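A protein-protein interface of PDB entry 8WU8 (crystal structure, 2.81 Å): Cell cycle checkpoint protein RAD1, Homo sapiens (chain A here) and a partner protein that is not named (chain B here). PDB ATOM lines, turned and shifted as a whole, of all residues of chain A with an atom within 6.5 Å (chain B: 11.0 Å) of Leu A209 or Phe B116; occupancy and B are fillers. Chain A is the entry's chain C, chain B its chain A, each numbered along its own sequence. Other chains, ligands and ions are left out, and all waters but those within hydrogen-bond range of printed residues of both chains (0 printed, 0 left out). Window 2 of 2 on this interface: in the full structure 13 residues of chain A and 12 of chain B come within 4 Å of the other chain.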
ATOM      1  N   ILE A 157       2.543 -17.459 -17.290  1.00  0.00           N
ATOM      2  CA  ILE A 157       2.087 -17.791 -18.635  1.00  0.00           C
ATOM      3  C   ILE A 157       0.679 -17.246 -18.868  1.00  0.00           C
ATOM      4  O   ILE A 157      -0.272 -17.658 -18.199  1.00  0.00           O
ATOM      5  CB  ILE A 157       2.105 -19.314 -18.884  1.00  0.00           C
ATOM      6  CG1 ILE A 157       3.495 -19.887 -18.597  1.00  0.00           C
ATOM      7  CG2 ILE A 157       1.707 -19.610 -20.316  1.00  0.00           C
ATOM      8  CD1 ILE A 157       3.568 -21.384 -18.738  1.00  0.00           C
ATOM      9  N   LEU A 158       0.557 -16.318 -19.814  1.00  0.00           N
ATOM     10  CA  LEU A 158      -0.678 -15.567 -20.008  1.00  0.00           C
ATOM     11  C   LEU A 158      -1.293 -15.829 -21.381  1.00  0.00           C
ATOM     12  O   LEU A 158      -0.593 -16.216 -22.315  1.00  0.00           O
ATOM     13  CB  LEU A 158      -0.400 -14.071 -19.832  1.00  0.00           C
ATOM     14  CG  LEU A 158      -1.543 -13.159 -19.398  1.00  0.00           C
ATOM     15  CD1 LEU A 158      -2.018 -13.566 -18.020  1.00  0.00           C
ATOM     16  CD2 LEU A 158      -1.091 -11.707 -19.403  1.00  0.00           C
ATOM     17  N   GLN A 159      -2.600 -15.617 -21.500  1.00  0.00           N
ATOM     18  CA  GLN A 159      -3.255 -15.672 -22.802  1.00  0.00           C
ATOM     19  C   GLN A 159      -2.975 -14.382 -23.560  1.00  0.00           C
ATOM     20  O   GLN A 159      -3.282 -13.290 -23.082  1.00  0.00           O
ATOM     21  CB  GLN A 159      -4.763 -15.896 -22.655  1.00  0.00           C
ATOM     22  CG  GLN A 159      -5.127 -17.251 -22.076  1.00  0.00           C
ATOM     23  CD  GLN A 159      -6.622 -17.502 -22.056  1.00  0.00           C
ATOM     24  OE1 GLN A 159      -7.409 -16.681 -22.528  1.00  0.00           O
ATOM     25  NE2 GLN A 159      -7.021 -18.643 -21.508  1.00  0.00           N
ATOM     26  N   SER A 160      -2.386 -14.518 -24.743  1.00  0.00           N
ATOM     27  CA  SER A 160      -1.924 -13.370 -25.512  1.00  0.00           C
ATOM     28  C   SER A 160      -3.061 -12.425 -25.902  1.00  0.00           C
ATOM     29  O   SER A 160      -2.845 -11.224 -26.070  1.00  0.00           O
ATOM     30  CB  SER A 160      -1.188 -13.844 -26.770  1.00  0.00           C
ATOM     31  OG  SER A 160      -0.151 -14.754 -26.444  1.00  0.00           O
ATOM     32  N   GLU A 161      -4.268 -12.972 -26.015  1.00  0.00           N
ATOM     33  CA  GLU A 161      -5.423 -12.248 -26.542  1.00  0.00           C
ATOM     34  C   GLU A 161      -5.731 -10.939 -25.808  1.00  0.00           C
ATOM     35  O   GLU A 161      -6.171  -9.968 -26.424  1.00  0.00           O
ATOM     36  CB  GLU A 161      -6.655 -13.160 -26.514  1.00  0.00           C
ATOM     37  CG  GLU A 161      -7.755 -12.773 -27.496  1.00  0.00           C
ATOM     38  CD  GLU A 161      -8.802 -13.865 -27.660  1.00  0.00           C
ATOM     39  OE1 GLU A 161      -8.780 -14.838 -26.877  1.00  0.00           O
ATOM     40  OE2 GLU A 161      -9.644 -13.751 -28.576  1.00  0.00           O
ATOM     41  N   GLY A 162      -5.496 -10.910 -24.499  1.00  0.00           N
ATOM     42  CA  GLY A 162      -5.804  -9.736 -23.700  1.00  0.00           C
ATOM     43  C   GLY A 162      -4.624  -8.803 -23.489  1.00  0.00           C
ATOM     44  O   GLY A 162      -4.790  -7.668 -23.039  1.00  0.00           O
ATOM     45  N   LEU A 163      -3.432  -9.279 -23.825  1.00  0.00           N
ATOM     46  CA  LEU A 163      -2.212  -8.513 -23.601  1.00  0.00           C
ATOM     47  C   LEU A 163      -1.856  -7.644 -24.806  1.00  0.00           C
ATOM     48  O   LEU A 163      -1.037  -6.730 -24.703  1.00  0.00           O
ATOM     49  CB  LEU A 163      -1.054  -9.457 -23.267  1.00  0.00           C
ATOM     50  CG  LEU A 163       0.086  -8.865 -22.439  1.00  0.00           C
ATOM     51  CD1 LEU A 163      -0.419  -8.447 -21.064  1.00  0.00           C
ATOM     52  CD2 LEU A 163       1.238  -9.852 -22.318  1.00  0.00           C
ATOM     53  N   TYR A 203      -2.980  -7.611 -13.378  1.00  0.00           N
ATOM     54  CA  TYR A 203      -3.456  -8.957 -13.659  1.00  0.00           C
ATOM     55  C   TYR A 203      -3.440  -9.787 -12.380  1.00  0.00           C
ATOM     56  O   TYR A 203      -2.368 -10.126 -11.878  1.00  0.00           O
ATOM     57  CB  TYR A 203      -2.594  -9.628 -14.728  1.00  0.00           C
ATOM     58  CG  TYR A 203      -2.913  -9.223 -16.150  1.00  0.00           C
ATOM     59  CD1 TYR A 203      -2.513  -7.992 -16.652  1.00  0.00           C
ATOM     60  CD2 TYR A 203      -3.599 -10.083 -16.996  1.00  0.00           C
ATOM     61  CE1 TYR A 203      -2.799  -7.626 -17.953  1.00  0.00           C
ATOM     62  CE2 TYR A 203      -3.889  -9.727 -18.296  1.00  0.00           C
ATOM     63  CZ  TYR A 203      -3.488  -8.499 -18.770  1.00  0.00           C
ATOM     64  OH  TYR A 203      -3.778  -8.143 -20.067  1.00  0.00           O
ATOM     65  N   PRO A 204      -4.624 -10.111 -11.841  1.00  0.00           N
ATOM     66  CA  PRO A 204      -4.672 -10.982 -10.662  1.00  0.00           C
ATOM     67  C   PRO A 204      -4.160 -12.378 -11.003  1.00  0.00           C
ATOM     68  O   PRO A 204      -4.272 -12.792 -12.156  1.00  0.00           O
ATOM     69  CB  PRO A 204      -6.160 -11.005 -10.298  1.00  0.00           C
ATOM     70  CG  PRO A 204      -6.867 -10.688 -11.575  1.00  0.00           C
ATOM     71  CD  PRO A 204      -5.969  -9.731 -12.309  1.00  0.00           C
ATOM     72  N   ASP A 206      -5.387 -15.078  -9.981  1.00  0.00           N
ATOM     73  CA  ASP A 206      -6.550 -15.949 -10.102  1.00  0.00           C
ATOM     74  C   ASP A 206      -7.352 -15.640 -11.361  1.00  0.00           C
ATOM     75  O   ASP A 206      -8.470 -16.128 -11.529  1.00  0.00           O
ATOM     76  CB  ASP A 206      -7.446 -15.825  -8.868  1.00  0.00           C
ATOM     77  CG  ASP A 206      -6.800 -16.395  -7.619  1.00  0.00           C
ATOM     78  OD1 ASP A 206      -5.895 -17.245  -7.755  1.00  0.00           O
ATOM     79  OD2 ASP A 206      -7.198 -15.997  -6.502  1.00  0.00           O
ATOM     80  N   SER A 207      -6.776 -14.831 -12.244  1.00  0.00           N
ATOM     81  CA  SER A 207      -7.447 -14.473 -13.486  1.00  0.00           C
ATOM     82  C   SER A 207      -7.509 -15.667 -14.426  1.00  0.00           C
ATOM     83  O   SER A 207      -6.620 -16.519 -14.429  1.00  0.00           O
ATOM     84  CB  SER A 207      -6.742 -13.300 -14.170  1.00  0.00           C
ATOM     85  OG  SER A 207      -7.439 -12.901 -15.338  1.00  0.00           O
ATOM     86  N   ASP A 208      -8.569 -15.722 -15.223  1.00  0.00           N
ATOM     87  CA  ASP A 208      -8.753 -16.805 -16.177  1.00  0.00           C
ATOM     88  C   ASP A 208      -7.791 -16.653 -17.350  1.00  0.00           C
ATOM     89  O   ASP A 208      -7.530 -17.611 -18.079  1.00  0.00           O
ATOM     90  CB  ASP A 208     -10.202 -16.841 -16.664  1.00  0.00           C
ATOM     91  CG  ASP A 208     -11.183 -17.119 -15.540  1.00  0.00           C
ATOM     92  OD1 ASP A 208     -10.844 -17.917 -14.640  1.00  0.00           O
ATOM     93  OD2 ASP A 208     -12.288 -16.536 -15.552  1.00  0.00           O
ATOM     94  N   LEU A 209      -7.267 -15.444 -17.521  1.00  0.00           N
ATOM     95  CA  LEU A 209      -6.259 -15.180 -18.541  1.00  0.00           C
ATOM     96  C   LEU A 209      -4.933 -15.828 -18.157  1.00  0.00           C
ATOM     97  O   LEU A 209      -4.112 -16.145 -19.017  1.00  0.00           O
ATOM     98  CB  LEU A 209      -6.079 -13.675 -18.742  1.00  0.00           C
ATOM     99  CG  LEU A 209      -7.323 -12.923 -19.213  1.00  0.00           C
ATOM    100  CD1 LEU A 209      -7.021 -11.447 -19.409  1.00  0.00           C
ATOM    101  CD2 LEU A 209      -7.861 -13.537 -20.493  1.00  0.00           C
ATOM    102  N   MET A 210      -4.735 -16.022 -16.856  1.00  0.00           N
ATOM    103  CA  MET A 210      -3.538 -16.677 -16.343  1.00  0.00           C
ATOM    104  C   MET A 210      -3.600 -18.177 -16.574  1.00  0.00           C
ATOM    105  O   MET A 210      -4.583 -18.830 -16.223  1.00  0.00           O
ATOM    106  CB  MET A 210      -3.361 -16.391 -14.851  1.00  0.00           C
ATOM    107  CG  MET A 210      -2.831 -15.008 -14.533  1.00  0.00           C
ATOM    108  SD  MET A 210      -1.056 -14.890 -14.804  1.00  0.00           S
ATOM    109  CE  MET A 210      -0.763 -13.180 -14.354  1.00  0.00           C
ATOM    110  N   GLU A 211      -2.545 -18.718 -17.170  1.00  0.00           N
ATOM    111  CA  GLU A 211      -2.432 -20.155 -17.359  1.00  0.00           C
ATOM    112  C   GLU A 211      -1.504 -20.739 -16.300  1.00  0.00           C
ATOM    113  O   GLU A 211      -1.711 -21.852 -15.819  1.00  0.00           O
ATOM    114  CB  GLU A 211      -1.919 -20.476 -18.765  1.00  0.00           C
ATOM    115  CG  GLU A 211      -2.784 -19.916 -19.884  1.00  0.00           C
ATOM    116  CD  GLU A 211      -4.163 -20.549 -19.933  1.00  0.00           C
ATOM    117  OE1 GLU A 211      -4.243 -21.787 -20.075  1.00  0.00           O
ATOM    118  OE2 GLU A 211      -5.165 -19.813 -19.823  1.00  0.00           O
ATOM    119  N   ALA A 212      -0.485 -19.970 -15.937  1.00  0.00           N
ATOM    120  CA  ALA A 212       0.471 -20.390 -14.923  1.00  0.00           C
ATOM    121  C   ALA A 212       1.032 -19.181 -14.173  1.00  0.00           C
ATOM    122  O   ALA A 212       1.377 -18.167 -14.778  1.00  0.00           O
ATOM    123  CB  ALA A 212       1.594 -21.193 -15.555  1.00  0.00           C
ATOM    124  N   LYS A 240      -0.627 -18.237 -26.422  1.00  0.00           N
ATOM    125  CA  LYS A 240      -0.148 -17.928 -25.080  1.00  0.00           C
ATOM    126  C   LYS A 240       1.260 -17.339 -25.113  1.00  0.00           C
ATOM    127  O   LYS A 240       2.026 -17.583 -26.044  1.00  0.00           O
ATOM    128  CB  LYS A 240      -0.178 -19.179 -24.198  1.00  0.00           C
ATOM    129  CG  LYS A 240      -1.552 -19.490 -23.626  1.00  0.00           C
ATOM    130  CD  LYS A 240      -2.089 -20.817 -24.137  1.00  0.00           C
ATOM    131  CE  LYS A 240      -1.254 -21.980 -23.628  1.00  0.00           C
ATOM    132  NZ  LYS A 240      -1.802 -23.287 -24.079  1.00  0.00           N
ATOM    133  N   MET B  89     -13.097  -1.696 -27.748  1.00  0.00           N
ATOM    134  CA  MET B  89     -12.451  -2.249 -26.559  1.00  0.00           C
ATOM    135  C   MET B  89     -13.113  -1.748 -25.283  1.00  0.00           C
ATOM    136  O   MET B  89     -12.898  -2.301 -24.206  1.00  0.00           O
ATOM    137  CB  MET B  89     -10.964  -1.899 -26.542  1.00  0.00           C
ATOM    138  CG  MET B  89     -10.060  -3.013 -27.025  1.00  0.00           C
ATOM    139  SD  MET B  89      -8.569  -2.368 -27.805  1.00  0.00           S
ATOM    140  CE  MET B  89      -9.182  -1.961 -29.437  1.00  0.00           C
ATOM    141  N   LYS B  92     -16.525  -4.154 -25.252  1.00  0.00           N
ATOM    142  CA  LYS B  92     -16.232  -5.563 -25.038  1.00  0.00           C
ATOM    143  C   LYS B  92     -15.632  -5.858 -23.663  1.00  0.00           C
ATOM    144  O   LYS B  92     -16.054  -6.796 -22.986  1.00  0.00           O
ATOM    145  CB  LYS B  92     -15.288  -6.067 -26.134  1.00  0.00           C
ATOM    146  CG  LYS B  92     -15.898  -6.070 -27.533  1.00  0.00           C
ATOM    147  CD  LYS B  92     -14.840  -6.340 -28.599  1.00  0.00           C
ATOM    148  CE  LYS B  92     -15.401  -6.171 -30.007  1.00  0.00           C
ATOM    149  NZ  LYS B  92     -14.338  -6.262 -31.051  1.00  0.00           N
ATOM    150  N   THR B  93     -14.654  -5.056 -23.252  1.00  0.00           N
ATOM    151  CA  THR B  93     -13.886  -5.359 -22.046  1.00  0.00           C
ATOM    152  C   THR B  93     -14.323  -4.568 -20.812  1.00  0.00           C
ATOM    153  O   THR B  93     -14.559  -5.145 -19.749  1.00  0.00           O
ATOM    154  CB  THR B  93     -12.380  -5.108 -22.272  1.00  0.00           C
ATOM    155  OG1 THR B  93     -12.152  -3.714 -22.503  1.00  0.00           O
ATOM    156  CG2 THR B  93     -11.881  -5.902 -23.470  1.00  0.00           C
ATOM    157  N   VAL B  94     -14.429  -3.251 -20.952  1.00  0.00           N
ATOM    158  CA  VAL B  94     -14.693  -2.387 -19.806  1.00  0.00           C
ATOM    159  C   VAL B  94     -16.109  -2.550 -19.254  1.00  0.00           C
ATOM    160  O   VAL B  94     -17.095  -2.288 -19.947  1.00  0.00           O
ATOM    161  CB  VAL B  94     -14.469  -0.910 -20.162  1.00  0.00           C
ATOM    162  CG1 VAL B  94     -14.648  -0.042 -18.929  1.00  0.00           C
ATOM    163  CG2 VAL B  94     -13.086  -0.716 -20.756  1.00  0.00           C
ATOM    164  N   GLU B  95     -16.196  -2.990 -18.002  1.00  0.00           N
ATOM    165  CA  GLU B  95     -17.471  -3.093 -17.300  1.00  0.00           C
ATOM    166  C   GLU B  95     -17.808  -1.787 -16.591  1.00  0.00           C
ATOM    167  O   GLU B  95     -18.825  -1.152 -16.874  1.00  0.00           O
ATOM    168  CB  GLU B  95     -17.439  -4.231 -16.279  1.00  0.00           C
ATOM    169  CG  GLU B  95     -17.285  -5.615 -16.871  1.00  0.00           C
ATOM    170  CD  GLU B  95     -17.199  -6.684 -15.799  1.00  0.00           C
ATOM    171  OE1 GLU B  95     -16.982  -6.325 -14.621  1.00  0.00           O
ATOM    172  OE2 GLU B  95     -17.350  -7.879 -16.131  1.00  0.00           O
ATOM    173  N   LYS B  96     -16.939  -1.398 -15.663  1.00  0.00           N
ATOM    174  CA  LYS B  96     -17.130  -0.182 -14.889  1.00  0.00           C
ATOM    175  C   LYS B  96     -15.990   0.799 -15.127  1.00  0.00           C
ATOM    176  O   LYS B  96     -14.841   0.399 -15.306  1.00  0.00           O
ATOM    177  CB  LYS B  96     -17.248  -0.513 -13.399  1.00  0.00           C
ATOM    178  CG  LYS B  96     -18.345  -1.518 -13.089  1.00  0.00           C
ATOM    179  CD  LYS B  96     -18.542  -1.707 -11.599  1.00  0.00           C
ATOM    180  CE  LYS B  96     -19.698  -2.656 -11.323  1.00  0.00           C
ATOM    181  NZ  LYS B  96     -19.943  -2.834  -9.864  1.00  0.00           N
ATOM    182  N   LEU B 112     -10.274   1.586 -15.129  1.00  0.00           N
ATOM    183  CA  LEU B 112     -11.105   0.749 -15.980  1.00  0.00           C
ATOM    184  C   LEU B 112     -11.151  -0.679 -15.444  1.00  0.00           C
ATOM    185  O   LEU B 112     -10.172  -1.416 -15.553  1.00  0.00           O
ATOM    186  CB  LEU B 112     -10.579   0.749 -17.416  1.00  0.00           C
ATOM    187  CG  LEU B 112     -10.351   2.108 -18.081  1.00  0.00           C
ATOM    188  CD1 LEU B 112      -9.969   1.937 -19.550  1.00  0.00           C
ATOM    189  CD2 LEU B 112     -11.581   2.990 -17.939  1.00  0.00           C
ATOM    190  N   HIS B 113     -12.284  -1.065 -14.863  1.00  0.00           N
ATOM    191  CA  HIS B 113     -12.458  -2.431 -14.372  1.00  0.00           C
ATOM    192  C   HIS B 113     -12.907  -3.364 -15.487  1.00  0.00           C
ATOM    193  O   HIS B 113     -14.093  -3.448 -15.800  1.00  0.00           O
ATOM    194  CB  HIS B 113     -13.462  -2.473 -13.222  1.00  0.00           C
ATOM    195  CG  HIS B 113     -12.943  -1.882 -11.950  1.00  0.00           C
ATOM    196  ND1 HIS B 113     -12.953  -0.526 -11.703  1.00  0.00           N
ATOM    197  CD2 HIS B 113     -12.387  -2.460 -10.860  1.00  0.00           C
ATOM    198  CE1 HIS B 113     -12.431  -0.295 -10.512  1.00  0.00           C
ATOM    199  NE2 HIS B 113     -12.079  -1.452  -9.980  1.00  0.00           N
ATOM    200  N   CYS B 114     -11.949  -4.068 -16.077  1.00  0.00           N
ATOM    201  CA  CYS B 114     -12.229  -4.947 -17.203  1.00  0.00           C
ATOM    202  C   CYS B 114     -12.601  -6.345 -16.731  1.00  0.00           C
ATOM    203  O   CYS B 114     -12.707  -6.598 -15.529  1.00  0.00           O
ATOM    204  CB  CYS B 114     -11.021  -5.009 -18.135  1.00  0.00           C
ATOM    205  SG  CYS B 114     -10.228  -3.407 -18.404  1.00  0.00           S
ATOM    206  N   LYS B 115     -12.795  -7.249 -17.686  1.00  0.00           N
ATOM    207  CA  LYS B 115     -13.139  -8.633 -17.385  1.00  0.00           C
ATOM    208  C   LYS B 115     -11.987  -9.367 -16.708  1.00  0.00           C
ATOM    209  O   LYS B 115     -10.850  -8.892 -16.709  1.00  0.00           O
ATOM    210  CB  LYS B 115     -13.536  -9.381 -18.661  1.00  0.00           C
ATOM    211  CG  LYS B 115     -14.841  -8.929 -19.293  1.00  0.00           C
ATOM    212  CD  LYS B 115     -15.168  -9.787 -20.506  1.00  0.00           C
ATOM    213  CE  LYS B 115     -16.495  -9.397 -21.135  1.00  0.00           C
ATOM    214  NZ  LYS B 115     -16.814 -10.244 -22.321  1.00  0.00           N
ATOM    215  N   PHE B 116     -12.304 -10.521 -16.124  1.00  0.00           N
ATOM    216  CA  PHE B 116     -11.309 -11.453 -15.590  1.00  0.00           C
ATOM    217  C   PHE B 116     -10.435 -10.833 -14.504  1.00  0.00           C
ATOM    218  O   PHE B 116      -9.323 -11.299 -14.249  1.00  0.00           O
ATOM    219  CB  PHE B 116     -10.432 -11.986 -16.726  1.00  0.00           C
ATOM    220  CG  PHE B 116     -11.204 -12.338 -17.968  1.00  0.00           C
ATOM    221  CD1 PHE B 116     -12.351 -13.113 -17.891  1.00  0.00           C
ATOM    222  CD2 PHE B 116     -10.794 -11.877 -19.207  1.00  0.00           C
ATOM    223  CE1 PHE B 116     -13.066 -13.431 -19.027  1.00  0.00           C
ATOM    224  CE2 PHE B 116     -11.505 -12.193 -20.349  1.00  0.00           C
ATOM    225  CZ  PHE B 116     -12.645 -12.971 -20.258  1.00  0.00           C
ATOM    226  N   GLY B 117     -10.946  -9.782 -13.867  1.00  0.00           N
ATOM    227  CA  GLY B 117     -10.249  -9.132 -12.772  1.00  0.00           C
ATOM    228  C   GLY B 117      -9.248  -8.093 -13.226  1.00  0.00           C
ATOM    229  O   GLY B 117      -8.670  -7.380 -12.407  1.00  0.00           O
ATOM    230  N   VAL B 118      -9.044  -8.008 -14.538  1.00  0.00           N
ATOM    231  CA  VAL B 118      -8.073  -7.079 -15.106  1.00  0.00           C
ATOM    232  C   VAL B 118      -8.492  -5.638 -14.849  1.00  0.00           C
ATOM    233  O   VAL B 118      -9.641  -5.265 -15.085  1.00  0.00           O
ATOM    234  CB  VAL B 118      -7.896  -7.298 -16.622  1.00  0.00           C
ATOM    235  CG1 VAL B 118      -6.908  -6.296 -17.197  1.00  0.00           C
ATOM    236  CG2 VAL B 118      -7.432  -8.719 -16.900  1.00  0.00           C
ATOM    237  N   ARG B 119      -7.556  -4.837 -14.352  1.00  0.00           N
ATOM    238  CA  ARG B 119      -7.823  -3.438 -14.048  1.00  0.00           C
ATOM    239  C   ARG B 119      -6.830  -2.524 -14.752  1.00  0.00           C
ATOM    240  O   ARG B 119      -5.619  -2.718 -14.658  1.00  0.00           O
ATOM    241  CB  ARG B 119      -7.776  -3.198 -12.538  1.00  0.00           C
ATOM    242  CG  ARG B 119      -7.827  -1.731 -12.142  1.00  0.00           C
ATOM    243  CD  ARG B 119      -7.475  -1.539 -10.675  1.00  0.00           C
ATOM    244  NE  ARG B 119      -8.403  -2.239  -9.793  1.00  0.00           N
ATOM    245  CZ  ARG B 119      -8.332  -2.222  -8.465  1.00  0.00           C
ATOM    246  NH1 ARG B 119      -7.372  -1.536  -7.859  1.00  0.00           N
ATOM    247  NH2 ARG B 119      -9.222  -2.889  -7.742  1.00  0.00           N
ATOM    248  N   LYS B 120      -7.356  -1.533 -15.466  1.00  0.00           N
ATOM    249  CA  LYS B 120      -6.534  -0.515 -16.106  1.00  0.00           C
ATOM    250  C   LYS B 120      -6.668   0.785 -15.326  1.00  0.00           C
ATOM    251  O   LYS B 120      -7.780   1.211 -15.017  1.00  0.00           O
ATOM    252  CB  LYS B 120      -6.952  -0.316 -17.563  1.00  0.00           C
ATOM    253  CG  LYS B 120      -6.122   0.700 -18.331  1.00  0.00           C
ATOM    254  CD  LYS B 120      -4.760   0.140 -18.701  1.00  0.00           C
ATOM    255  CE  LYS B 120      -4.027   1.071 -19.655  1.00  0.00           C
ATOM    256  NZ  LYS B 120      -2.677   0.558 -20.015  1.00  0.00           N
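O of Phe B116 lies within hydrogen-bond range of OG of Ser A207 (2.7 Å).
The side-chain hydroxyl (OG) of Ser A207 sits close to the backbone NH (N) of Leu A209. The backbone carbonyl oxygen (O) of Gly A162 is in hydrogen-bond range of the side-chain hydroxyl (OH) of Tyr A203 (3.2 Å). The backbone carbonyl oxygen of Leu A209 is in hydrogen-bond range of the backbone NH of Gln A159, at 3.0 Å.
CG2 of Val B118 touches CE2 of Tyr A203 (3.9 Å). Phe B116 touches Pro A204 (O to CG, 3.7 Å). Gly B117 touches Pro A204. CD2 of Leu A209 touches CD2 of Phe B116, at 3.6 Å. Val B118 touches Leu A209 (CG2 to CD1, 3.7 Å).
No residue of chain B comes within 4 Å of Leu A158. No residue of chain B comes within 4 Å of Gln A159. No residue of chain B comes within 4 Å of Gly A162. Of the printed residues of chain B, Tyr A203 touches Val B118. Ser A207 touches just one residue of chain B: Phe B116 (2.7 Å). No residue of chain B comes within 4 Å of Asp A208. Leu A209 touches just these residues of chain B: Phe B116 (3.6 Å) and Val B118 (3.7 Å). No residue of chain B comes within 4 Å of Met A210. Phe B116 touches just these residues of chain A: Pro A204 (3.7 Å), Ser A207 (2.7 Å) and Leu A209 (3.6 Å). Printed residues of chain A within 4 Å of Gly B117: Pro A204. Of the printed residues of chain A, Val B118 touches Tyr A203 (3.9 Å) and Leu A209 (3.7 Å). The nearest residue of chain B that does not touch Leu A209 is Lys B115 (5.3 Å). The nearest printed residue of chain B that does not touch Tyr A203 is Arg B119 (5.4 Å).
Of the 17 printed residues of chain A, 4 touch a printed residue of chain B. Hydrophobic or aromatic side chains of chain A within 4 Å of the printed part of chain B: Tyr A203, Pro A204 and Leu A209. Of the 15 printed residues of chain B, 3 touch a printed residue of chain A. Hydrophobic or aromatic side chains of chain B that line the printed part of chain A: Phe B116 and Val B118. Among the printed residues, 6 pairs touch across the chains. Among the printed residues, no Asp or Glu carboxylate lies within 4 Å of a Lys or Arg side-chain nitrogen of the other chain.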
